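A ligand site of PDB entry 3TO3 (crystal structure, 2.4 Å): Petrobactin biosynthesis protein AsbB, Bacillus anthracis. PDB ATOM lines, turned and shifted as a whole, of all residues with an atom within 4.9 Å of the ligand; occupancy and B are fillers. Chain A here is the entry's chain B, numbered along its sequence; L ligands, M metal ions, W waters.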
ATOM      1  N   GLY A 160       3.915  13.648 -24.216  1.00  0.00           N
ATOM      2  CA  GLY A 160       2.956  13.915 -23.164  1.00  0.00           C
ATOM      3  C   GLY A 160       3.170  15.320 -22.614  1.00  0.00           C
ATOM      4  O   GLY A 160       3.801  16.176 -23.226  1.00  0.00           O
ATOM      5  N   HIS A 161       2.645  15.540 -21.432  1.00  0.00           N
ATOM      6  CA  HIS A 161       2.521  16.883 -20.911  1.00  0.00           C
ATOM      7  C   HIS A 161       3.846  17.494 -20.449  1.00  0.00           C
ATOM      8  O   HIS A 161       4.619  16.866 -19.730  1.00  0.00           O
ATOM      9  CB  HIS A 161       1.516  16.871 -19.753  1.00  0.00           C
ATOM     10  CG  HIS A 161       0.755  18.146 -19.627  1.00  0.00           C
ATOM     11  ND1 HIS A 161       1.307  19.279 -19.068  1.00  0.00           N
ATOM     12  CD2 HIS A 161      -0.515  18.464 -19.983  1.00  0.00           C
ATOM     13  CE1 HIS A 161       0.401  20.244 -19.089  1.00  0.00           C
ATOM     14  NE2 HIS A 161      -0.708  19.780 -19.646  1.00  0.00           N
ATOM     15  N   PRO A 162       4.113  18.713 -20.922  1.00  0.00           N
ATOM     16  CA  PRO A 162       5.271  19.599 -20.647  1.00  0.00           C
ATOM     17  C   PRO A 162       5.245  20.246 -19.221  1.00  0.00           C
ATOM     18  O   PRO A 162       6.260  20.787 -18.759  1.00  0.00           O
ATOM     19  CB  PRO A 162       5.208  20.653 -21.771  1.00  0.00           C
ATOM     20  CG  PRO A 162       3.677  20.744 -22.079  1.00  0.00           C
ATOM     21  CD  PRO A 162       3.109  19.357 -21.802  1.00  0.00           C
ATOM     22  N   TYR A 167       3.347  12.696 -16.275  1.00  0.00           N
ATOM     23  CA  TYR A 167       2.554  12.796 -17.503  1.00  0.00           C
ATOM     24  C   TYR A 167       2.215  11.462 -18.157  1.00  0.00           C
ATOM     25  O   TYR A 167       1.479  11.409 -19.137  1.00  0.00           O
ATOM     26  CB  TYR A 167       3.359  13.655 -18.510  1.00  0.00           C
ATOM     27  CG  TYR A 167       4.844  13.280 -18.655  1.00  0.00           C
ATOM     28  CD1 TYR A 167       5.249  12.247 -19.499  1.00  0.00           C
ATOM     29  CD2 TYR A 167       5.831  13.933 -17.922  1.00  0.00           C
ATOM     30  CE1 TYR A 167       6.586  11.895 -19.628  1.00  0.00           C
ATOM     31  CE2 TYR A 167       7.190  13.580 -18.048  1.00  0.00           C
ATOM     32  CZ  TYR A 167       7.548  12.553 -18.910  1.00  0.00           C
ATOM     33  OH  TYR A 167       8.867  12.184 -19.054  1.00  0.00           O
ATOM     34  N   GLN A 282      -3.731  10.005 -28.286  1.00  0.00           N
ATOM     35  CA  GLN A 282      -2.983  10.458 -27.131  1.00  0.00           C
ATOM     36  C   GLN A 282      -3.731  10.229 -25.836  1.00  0.00           C
ATOM     37  O   GLN A 282      -3.108  10.085 -24.789  1.00  0.00           O
ATOM     38  CB  GLN A 282      -2.686  11.957 -27.223  1.00  0.00           C
ATOM     39  CG  GLN A 282      -1.510  12.321 -28.112  1.00  0.00           C
ATOM     40  CD  GLN A 282      -1.288  13.827 -28.179  1.00  0.00           C
ATOM     41  OE1 GLN A 282      -0.311  14.329 -27.628  1.00  0.00           O
ATOM     42  NE2 GLN A 282      -2.199  14.545 -28.860  1.00  0.00           N
ATOM     43  N   SER A 283      -5.057  10.217 -25.909  1.00  0.00           N
ATOM     44  CA  SER A 283      -5.918  10.101 -24.726  1.00  0.00           C
ATOM     45  C   SER A 283      -6.011   8.665 -24.231  1.00  0.00           C
ATOM     46  O   SER A 283      -6.260   8.409 -23.039  1.00  0.00           O
ATOM     47  CB  SER A 283      -7.302  10.722 -24.997  1.00  0.00           C
ATOM     48  OG  SER A 283      -8.393   9.795 -24.933  1.00  0.00           O
ATOM     49  N   ARG A 285      -8.225   6.397 -24.172  1.00  0.00           N
ATOM     50  CA  ARG A 285      -9.584   5.860 -24.058  1.00  0.00           C
ATOM     51  C   ARG A 285     -10.377   6.327 -25.273  1.00  0.00           C
ATOM     52  O   ARG A 285     -11.539   5.990 -25.437  1.00  0.00           O
ATOM     53  CB  ARG A 285     -10.244   6.246 -22.725  1.00  0.00           C
ATOM     54  CG  ARG A 285     -10.195   7.714 -22.465  1.00  0.00           C
ATOM     55  CD  ARG A 285     -11.118   8.107 -21.339  1.00  0.00           C
ATOM     56  NE  ARG A 285     -11.027   9.534 -21.084  1.00  0.00           N
ATOM     57  CZ  ARG A 285     -11.794  10.198 -20.226  1.00  0.00           C
ATOM     58  NH1 ARG A 285     -12.724   9.554 -19.548  1.00  0.00           N
ATOM     59  NH2 ARG A 285     -11.625  11.507 -20.053  1.00  0.00           N
ATOM     60  N   THR A 286      -9.746   7.123 -26.115  1.00  0.00           N
ATOM     61  CA  THR A 286     -10.368   7.566 -27.343  1.00  0.00           C
ATOM     62  C   THR A 286      -9.750   6.837 -28.519  1.00  0.00           C
ATOM     63  O   THR A 286      -8.575   6.933 -28.735  1.00  0.00           O
ATOM     64  CB  THR A 286     -10.139   9.059 -27.578  1.00  0.00           C
ATOM     65  OG1 THR A 286     -10.628   9.791 -26.438  1.00  0.00           O
ATOM     66  CG2 THR A 286     -10.868   9.509 -28.863  1.00  0.00           C
ATOM     67  N   LYS A 299     -14.999   7.158 -27.579  1.00  0.00           N
ATOM     68  CA  LYS A 299     -14.397   7.528 -26.307  1.00  0.00           C
ATOM     69  C   LYS A 299     -15.062   6.664 -25.258  1.00  0.00           C
ATOM     70  O   LYS A 299     -16.289   6.755 -25.038  1.00  0.00           O
ATOM     71  CB  LYS A 299     -14.558   9.017 -26.010  1.00  0.00           C
ATOM     72  CG  LYS A 299     -13.961   9.477 -24.686  1.00  0.00           C
ATOM     73  CD  LYS A 299     -14.000  11.000 -24.557  1.00  0.00           C
ATOM     74  CE  LYS A 299     -13.063  11.491 -23.464  1.00  0.00           C
ATOM     75  NZ  LYS A 299     -13.165  12.979 -23.263  1.00  0.00           N
ATOM     76  N   ASN A 306      -4.225   8.348 -15.002  1.00  0.00           N
ATOM     77  CA  ASN A 306      -3.245   9.117 -15.743  1.00  0.00           C
ATOM     78  C   ASN A 306      -3.344  10.557 -15.330  1.00  0.00           C
ATOM     79  O   ASN A 306      -4.417  11.167 -15.473  1.00  0.00           O
ATOM     80  CB  ASN A 306      -3.526   9.009 -17.224  1.00  0.00           C
ATOM     81  CG  ASN A 306      -2.387   8.417 -17.969  1.00  0.00           C
ATOM     82  OD1 ASN A 306      -1.283   8.331 -17.432  1.00  0.00           O
ATOM     83  ND2 ASN A 306      -2.631   8.002 -19.198  1.00  0.00           N
ATOM     84  N   THR A 307      -2.249  11.118 -14.836  1.00  0.00           N
ATOM     85  CA  THR A 307      -2.232  12.496 -14.360  1.00  0.00           C
ATOM     86  C   THR A 307      -3.134  12.676 -13.119  1.00  0.00           C
ATOM     87  O   THR A 307      -3.692  13.747 -12.901  1.00  0.00           O
ATOM     88  CB  THR A 307      -2.571  13.521 -15.489  1.00  0.00           C
ATOM     89  OG1 THR A 307      -1.917  14.767 -15.216  1.00  0.00           O
ATOM     90  CG2 THR A 307      -4.082  13.758 -15.632  1.00  0.00           C
ATOM     91  N   ARG A 311     -10.026   7.669 -15.505  1.00  0.00           N
ATOM     92  CA  ARG A 311     -10.377   7.818 -16.931  1.00  0.00           C
ATOM     93  C   ARG A 311     -11.816   7.334 -17.211  1.00  0.00           C
ATOM     94  O   ARG A 311     -12.174   6.891 -18.301  1.00  0.00           O
ATOM     95  CB  ARG A 311      -9.338   7.202 -17.868  1.00  0.00           C
ATOM     96  CG  ARG A 311      -7.967   7.906 -17.818  1.00  0.00           C
ATOM     97  CD  ARG A 311      -8.079   9.396 -18.157  1.00  0.00           C
ATOM     98  NE  ARG A 311      -8.364  10.222 -16.972  1.00  0.00           N
ATOM     99  CZ  ARG A 311      -8.858  11.465 -17.018  1.00  0.00           C
ATOM    100  NH1 ARG A 311      -9.127  12.042 -18.181  1.00  0.00           N
ATOM    101  NH2 ARG A 311      -9.080  12.126 -15.887  1.00  0.00           N
ATOM    102  N   ARG A 371     -17.665  10.319 -31.546  1.00  0.00           N
ATOM    103  CA  ARG A 371     -17.308  11.661 -31.995  1.00  0.00           C
ATOM    104  C   ARG A 371     -16.958  11.677 -33.498  1.00  0.00           C
ATOM    105  O   ARG A 371     -16.393  10.703 -34.006  1.00  0.00           O
ATOM    106  CB  ARG A 371     -16.169  12.218 -31.133  1.00  0.00           C
ATOM    107  CG  ARG A 371     -15.293  13.203 -31.813  1.00  0.00           C
ATOM    108  CD  ARG A 371     -14.567  14.090 -30.801  1.00  0.00           C
ATOM    109  NE  ARG A 371     -13.580  13.394 -30.005  1.00  0.00           N
ATOM    110  CZ  ARG A 371     -13.372  13.622 -28.717  1.00  0.00           C
ATOM    111  NH1 ARG A 371     -14.086  14.527 -28.065  1.00  0.00           N
ATOM    112  NH2 ARG A 371     -12.438  12.950 -28.059  1.00  0.00           N
ATOM    113  N   ASN A 388      -0.844  20.498 -29.383  1.00  0.00           N
ATOM    114  CA  ASN A 388       0.402  20.356 -28.631  1.00  0.00           C
ATOM    115  C   ASN A 388       1.581  19.818 -29.484  1.00  0.00           C
ATOM    116  O   ASN A 388       2.738  19.918 -29.092  1.00  0.00           O
ATOM    117  CB  ASN A 388       0.204  19.517 -27.367  1.00  0.00           C
ATOM    118  CG  ASN A 388      -0.181  18.073 -27.673  1.00  0.00           C
ATOM    119  OD1 ASN A 388      -0.994  17.796 -28.556  1.00  0.00           O
ATOM    120  ND2 ASN A 388       0.399  17.137 -26.926  1.00  0.00           N
ATOM    121  N   TYR A 391       4.443  22.590 -30.325  1.00  0.00           N
ATOM    122  CA  TYR A 391       5.605  22.731 -29.448  1.00  0.00           C
ATOM    123  C   TYR A 391       6.367  21.438 -29.140  1.00  0.00           C
ATOM    124  O   TYR A 391       7.248  21.443 -28.293  1.00  0.00           O
ATOM    125  CB  TYR A 391       5.308  23.560 -28.186  1.00  0.00           C
ATOM    126  CG  TYR A 391       3.987  23.275 -27.522  1.00  0.00           C
ATOM    127  CD1 TYR A 391       3.874  22.281 -26.537  1.00  0.00           C
ATOM    128  CD2 TYR A 391       2.845  24.011 -27.842  1.00  0.00           C
ATOM    129  CE1 TYR A 391       2.646  22.014 -25.882  1.00  0.00           C
ATOM    130  CE2 TYR A 391       1.590  23.738 -27.205  1.00  0.00           C
ATOM    131  CZ  TYR A 391       1.514  22.753 -26.219  1.00  0.00           C
ATOM    132  OH  TYR A 391       0.302  22.501 -25.586  1.00  0.00           O
ATOM    133  N   HIS A 439      -7.043  23.763 -23.693  1.00  0.00           N
ATOM    134  CA  HIS A 439      -5.697  23.239 -23.523  1.00  0.00           C
ATOM    135  C   HIS A 439      -5.223  22.615 -24.858  1.00  0.00           C
ATOM    136  O   HIS A 439      -5.976  22.565 -25.848  1.00  0.00           O
ATOM    137  CB  HIS A 439      -5.640  22.172 -22.431  1.00  0.00           C
ATOM    138  CG  HIS A 439      -6.046  22.651 -21.057  1.00  0.00           C
ATOM    139  ND1 HIS A 439      -7.114  22.115 -20.375  1.00  0.00           N
ATOM    140  CD2 HIS A 439      -5.495  23.565 -20.216  1.00  0.00           C
ATOM    141  CE1 HIS A 439      -7.221  22.697 -19.185  1.00  0.00           C
ATOM    142  NE2 HIS A 439      -6.246  23.573 -19.057  1.00  0.00           N
ATOM    143  N   GLY A 440      -3.994  22.122 -24.892  1.00  0.00           N
ATOM    144  CA  GLY A 440      -3.413  21.644 -26.126  1.00  0.00           C
ATOM    145  C   GLY A 440      -4.043  20.423 -26.778  1.00  0.00           C
ATOM    146  O   GLY A 440      -4.035  20.295 -28.001  1.00  0.00           O
ATOM    147  N   GLN A 441      -4.592  19.537 -25.961  1.00  0.00           N
ATOM    148  CA  GLN A 441      -5.091  18.264 -26.453  1.00  0.00           C
ATOM    149  C   GLN A 441      -6.532  18.390 -26.973  1.00  0.00           C
ATOM    150  O   GLN A 441      -7.070  17.437 -27.558  1.00  0.00           O
ATOM    151  CB  GLN A 441      -4.972  17.186 -25.369  1.00  0.00           C
ATOM    152  CG  GLN A 441      -4.588  15.794 -25.901  1.00  0.00           C
ATOM    153  CD  GLN A 441      -5.798  14.850 -26.052  1.00  0.00           C
ATOM    154  OE1 GLN A 441      -6.828  15.036 -25.391  1.00  0.00           O
ATOM    155  NE2 GLN A 441      -5.665  13.832 -26.914  1.00  0.00           N
ATOM    156  N   LYS A 458     -12.352  19.841 -29.890  1.00  0.00           N
ATOM    157  CA  LYS A 458     -12.974  18.608 -29.423  1.00  0.00           C
ATOM    158  C   LYS A 458     -12.994  18.575 -27.901  1.00  0.00           C
ATOM    159  O   LYS A 458     -12.453  19.496 -27.272  1.00  0.00           O
ATOM    160  CB  LYS A 458     -12.250  17.372 -29.978  1.00  0.00           C
ATOM    161  CG  LYS A 458     -10.733  17.299 -29.701  1.00  0.00           C
ATOM    162  CD  LYS A 458     -10.193  15.989 -30.306  1.00  0.00           C
ATOM    163  CE  LYS A 458      -8.725  15.683 -29.903  1.00  0.00           C
ATOM    164  NZ  LYS A 458      -8.581  15.360 -28.442  1.00  0.00           N
ATOM    165  N   ASP A 459     -13.586  17.507 -27.356  1.00  0.00           N
ATOM    166  CA  ASP A 459     -13.806  17.308 -25.927  1.00  0.00           C
ATOM    167  C   ASP A 459     -14.575  18.428 -25.219  1.00  0.00           C
ATOM    168  O   ASP A 459     -13.997  19.178 -24.431  1.00  0.00           O
ATOM    169  CB  ASP A 459     -12.471  17.026 -25.205  1.00  0.00           C
ATOM    170  CG  ASP A 459     -11.954  15.616 -25.458  1.00  0.00           C
ATOM    171  OD1 ASP A 459     -12.781  14.676 -25.515  1.00  0.00           O
ATOM    172  OD2 ASP A 459     -10.733  15.449 -25.613  1.00  0.00           O
ATOM    173  N   GLU A 462     -16.978  17.213 -20.929  1.00  0.00           N
ATOM    174  CA  GLU A 462     -16.447  17.507 -19.585  1.00  0.00           C
ATOM    175  C   GLU A 462     -16.035  18.952 -19.285  1.00  0.00           C
ATOM    176  O   GLU A 462     -16.357  19.479 -18.223  1.00  0.00           O
ATOM    177  CB  GLU A 462     -15.286  16.564 -19.259  1.00  0.00           C
ATOM    178  CG  GLU A 462     -14.216  16.487 -20.356  1.00  0.00           C
ATOM    179  CD  GLU A 462     -13.213  15.369 -20.133  1.00  0.00           C
ATOM    180  OE1 GLU A 462     -13.341  14.643 -19.104  1.00  0.00           O
ATOM    181  OE2 GLU A 462     -12.304  15.209 -20.977  1.00  0.00           O
HETATM  182  P1  LIG L   1      -9.609  12.853 -23.065  1.00  0.00           P
HETATM  183  O1  LIG L   1      -9.787  11.352 -23.029  1.00  0.00           O
HETATM  184  O2  LIG L   1     -10.614  13.499 -22.135  1.00  0.00           O
HETATM  185  O3  LIG L   1      -9.793  13.365 -24.538  1.00  0.00           O
HETATM  186  P2  LIG L   1      -7.618  12.941 -21.217  1.00  0.00           P
HETATM  187  O4  LIG L   1      -8.346  11.734 -20.668  1.00  0.00           O
HETATM  188  O5  LIG L   1      -7.763  14.170 -20.332  1.00  0.00           O
HETATM  189  O6  LIG L   1      -8.171  13.270 -22.630  1.00  0.00           O
HETATM  190  O7  LIG L   1      -6.105  12.549 -21.335  1.00  0.00           O
HETATM  191  C1  LIG L   1      -5.304  13.112 -22.308  1.00  0.00           C
HETATM  192  C2  LIG L   1      -3.893  13.012 -22.118  1.00  0.00           C
HETATM  193  O8  LIG L   1      -3.214  14.026 -22.933  1.00  0.00           O
HETATM  194  C3  LIG L   1      -3.543  13.319 -20.709  1.00  0.00           C
HETATM  195  O9  LIG L   1      -2.899  12.248 -20.142  1.00  0.00           O
HETATM  196  C4  LIG L   1      -2.652  14.492 -20.781  1.00  0.00           C
HETATM  197  O10 LIG L   1      -1.671  14.422 -19.848  1.00  0.00           O
HETATM  198  C5  LIG L   1      -2.101  14.379 -22.166  1.00  0.00           C
HETATM  199  N1  LIG L   1      -1.443  15.548 -22.671  1.00  0.00           N
HETATM  200  C6  LIG L   1      -0.209  15.554 -23.220  1.00  0.00           C
HETATM  201  N2  LIG L   1       0.080  16.808 -23.585  1.00  0.00           N
HETATM  202  C7  LIG L   1      -0.962  17.611 -23.280  1.00  0.00           C
HETATM  203  C8  LIG L   1      -1.193  18.993 -23.440  1.00  0.00           C
HETATM  204  N3  LIG L   1      -0.183  19.811 -24.041  1.00  0.00           N
HETATM  205  N4  LIG L   1      -2.368  19.509 -23.025  1.00  0.00           N
HETATM  206  C9  LIG L   1      -3.314  18.727 -22.459  1.00  0.00           C
HETATM  207  N5  LIG L   1      -3.116  17.396 -22.287  1.00  0.00           N
HETATM  208  C10 LIG L   1      -1.952  16.815 -22.685  1.00  0.00           C
HETATM  209 MG    MG M   1      -9.021  16.106 -23.686  1.00  0.00          MG
HETATM  210  O   HOH W   1      -8.657  16.625 -20.488  1.00  0.00           O
HETATM  211  O   HOH W   2       0.835  13.636 -20.572  1.00  0.00           O
HETATM  212  O   HOH W   3       0.758  21.602 -22.667  1.00  0.00           O
HETATM  213  O   HOH W   4       2.418  17.901 -25.115  1.00  0.00           O
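Gly 160 touches the ligand. His 161 touches the ligand. Thr 286 touches the ligand. Gly 440 touches the ligand (N to N4, 3.6 Å). OE1 of Gln 441 touches O3 of the ligand, 3.5 Å away. Hydrophobic or aromatic side chains that line the ligand: His 161. Of the 21 residues printed, 13 come within 4 Å of the ligand. Along chain A the residues within 4 Å of the ligand span positions 160 to 462. The nearest printed residue that does not touch the ligand is Pro 162 (4.01 Å).
Water W3 bridges a nitrogen (N3) of the ligand (2.4 Å) and the side-chain hydroxyl of Tyr 391 (3.1 Å). Water W2 lies within hydrogen-bond range of O10 of the ligand, O of Tyr 167 and N of His 161. Water W4 lies within hydrogen-bond range of the side-chain amide nitrogen of Asn 388 (2.8 Å), the backbone carbonyl oxygen of Gly 160 (2.9 Å) and a nitrogen (N2) of the ligand (3.0 Å).
OD2 of Asp 459 is in salt-bridge range of NZ of Lys 458, 3.6 Å away. The side-chain hydroxyl of Ser 283 sits close to the backbone NH of Arg 285, at 3.5 Å. The backbone carbonyl oxygen (O) of Gln 441 is in hydrogen-bond range of the side-chain amino group (NZ) of Lys 458 (2.7 Å). The side-chain amide nitrogen (ND2) of Asn 388 sits at hydrogen-bond distance from the side-chain amide oxygen (OE1) of Gln 282, at 3.0 Å. The guanidinium group (NH2) of Arg 285 lies within salt-bridge range of the side-chain carboxylate (OE1) of Glu 462, 3.7 Å away. The side-chain carboxylate (OD1) of Asp 459 lies within salt-bridge range of the side-chain amino group (NZ) of Lys 299, 2.8 Å away. OE2 of Glu 462 is in salt-bridge range of NZ of Lys 299. OD1 of Asp 459 lies within salt-bridge range of NH1 of Arg 371, at 2.9 Å.
The side-chain carboxylate of Asp 459 lies close to an oxygen (O3) of the ligand, 2.5 Å away. The side-chain hydroxyl of Ser 283 sits at hydrogen-bond distance from an oxygen (O1) of the ligand, at 2.8 Å. O1 of the ligand is in salt-bridge range of NE of Arg 285 (2.9 Å). OE2 of Glu 462 lies close to O2 of the ligand (2.7 Å). The side-chain hydroxyl (OH) of Tyr 391 lies within hydrogen-bond range of a nitrogen (N3) of the ligand, 3.1 Å away. O2 of the ligand lies within salt-bridge range of NZ of Lys 299. The side-chain amide nitrogen (ND2) of Asn 388 lies within hydrogen-bond range of a nitrogen (N2) of the ligand. O4 of the ligand lies within salt-bridge range of NH1 of Arg 311, 2.6 Å away.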
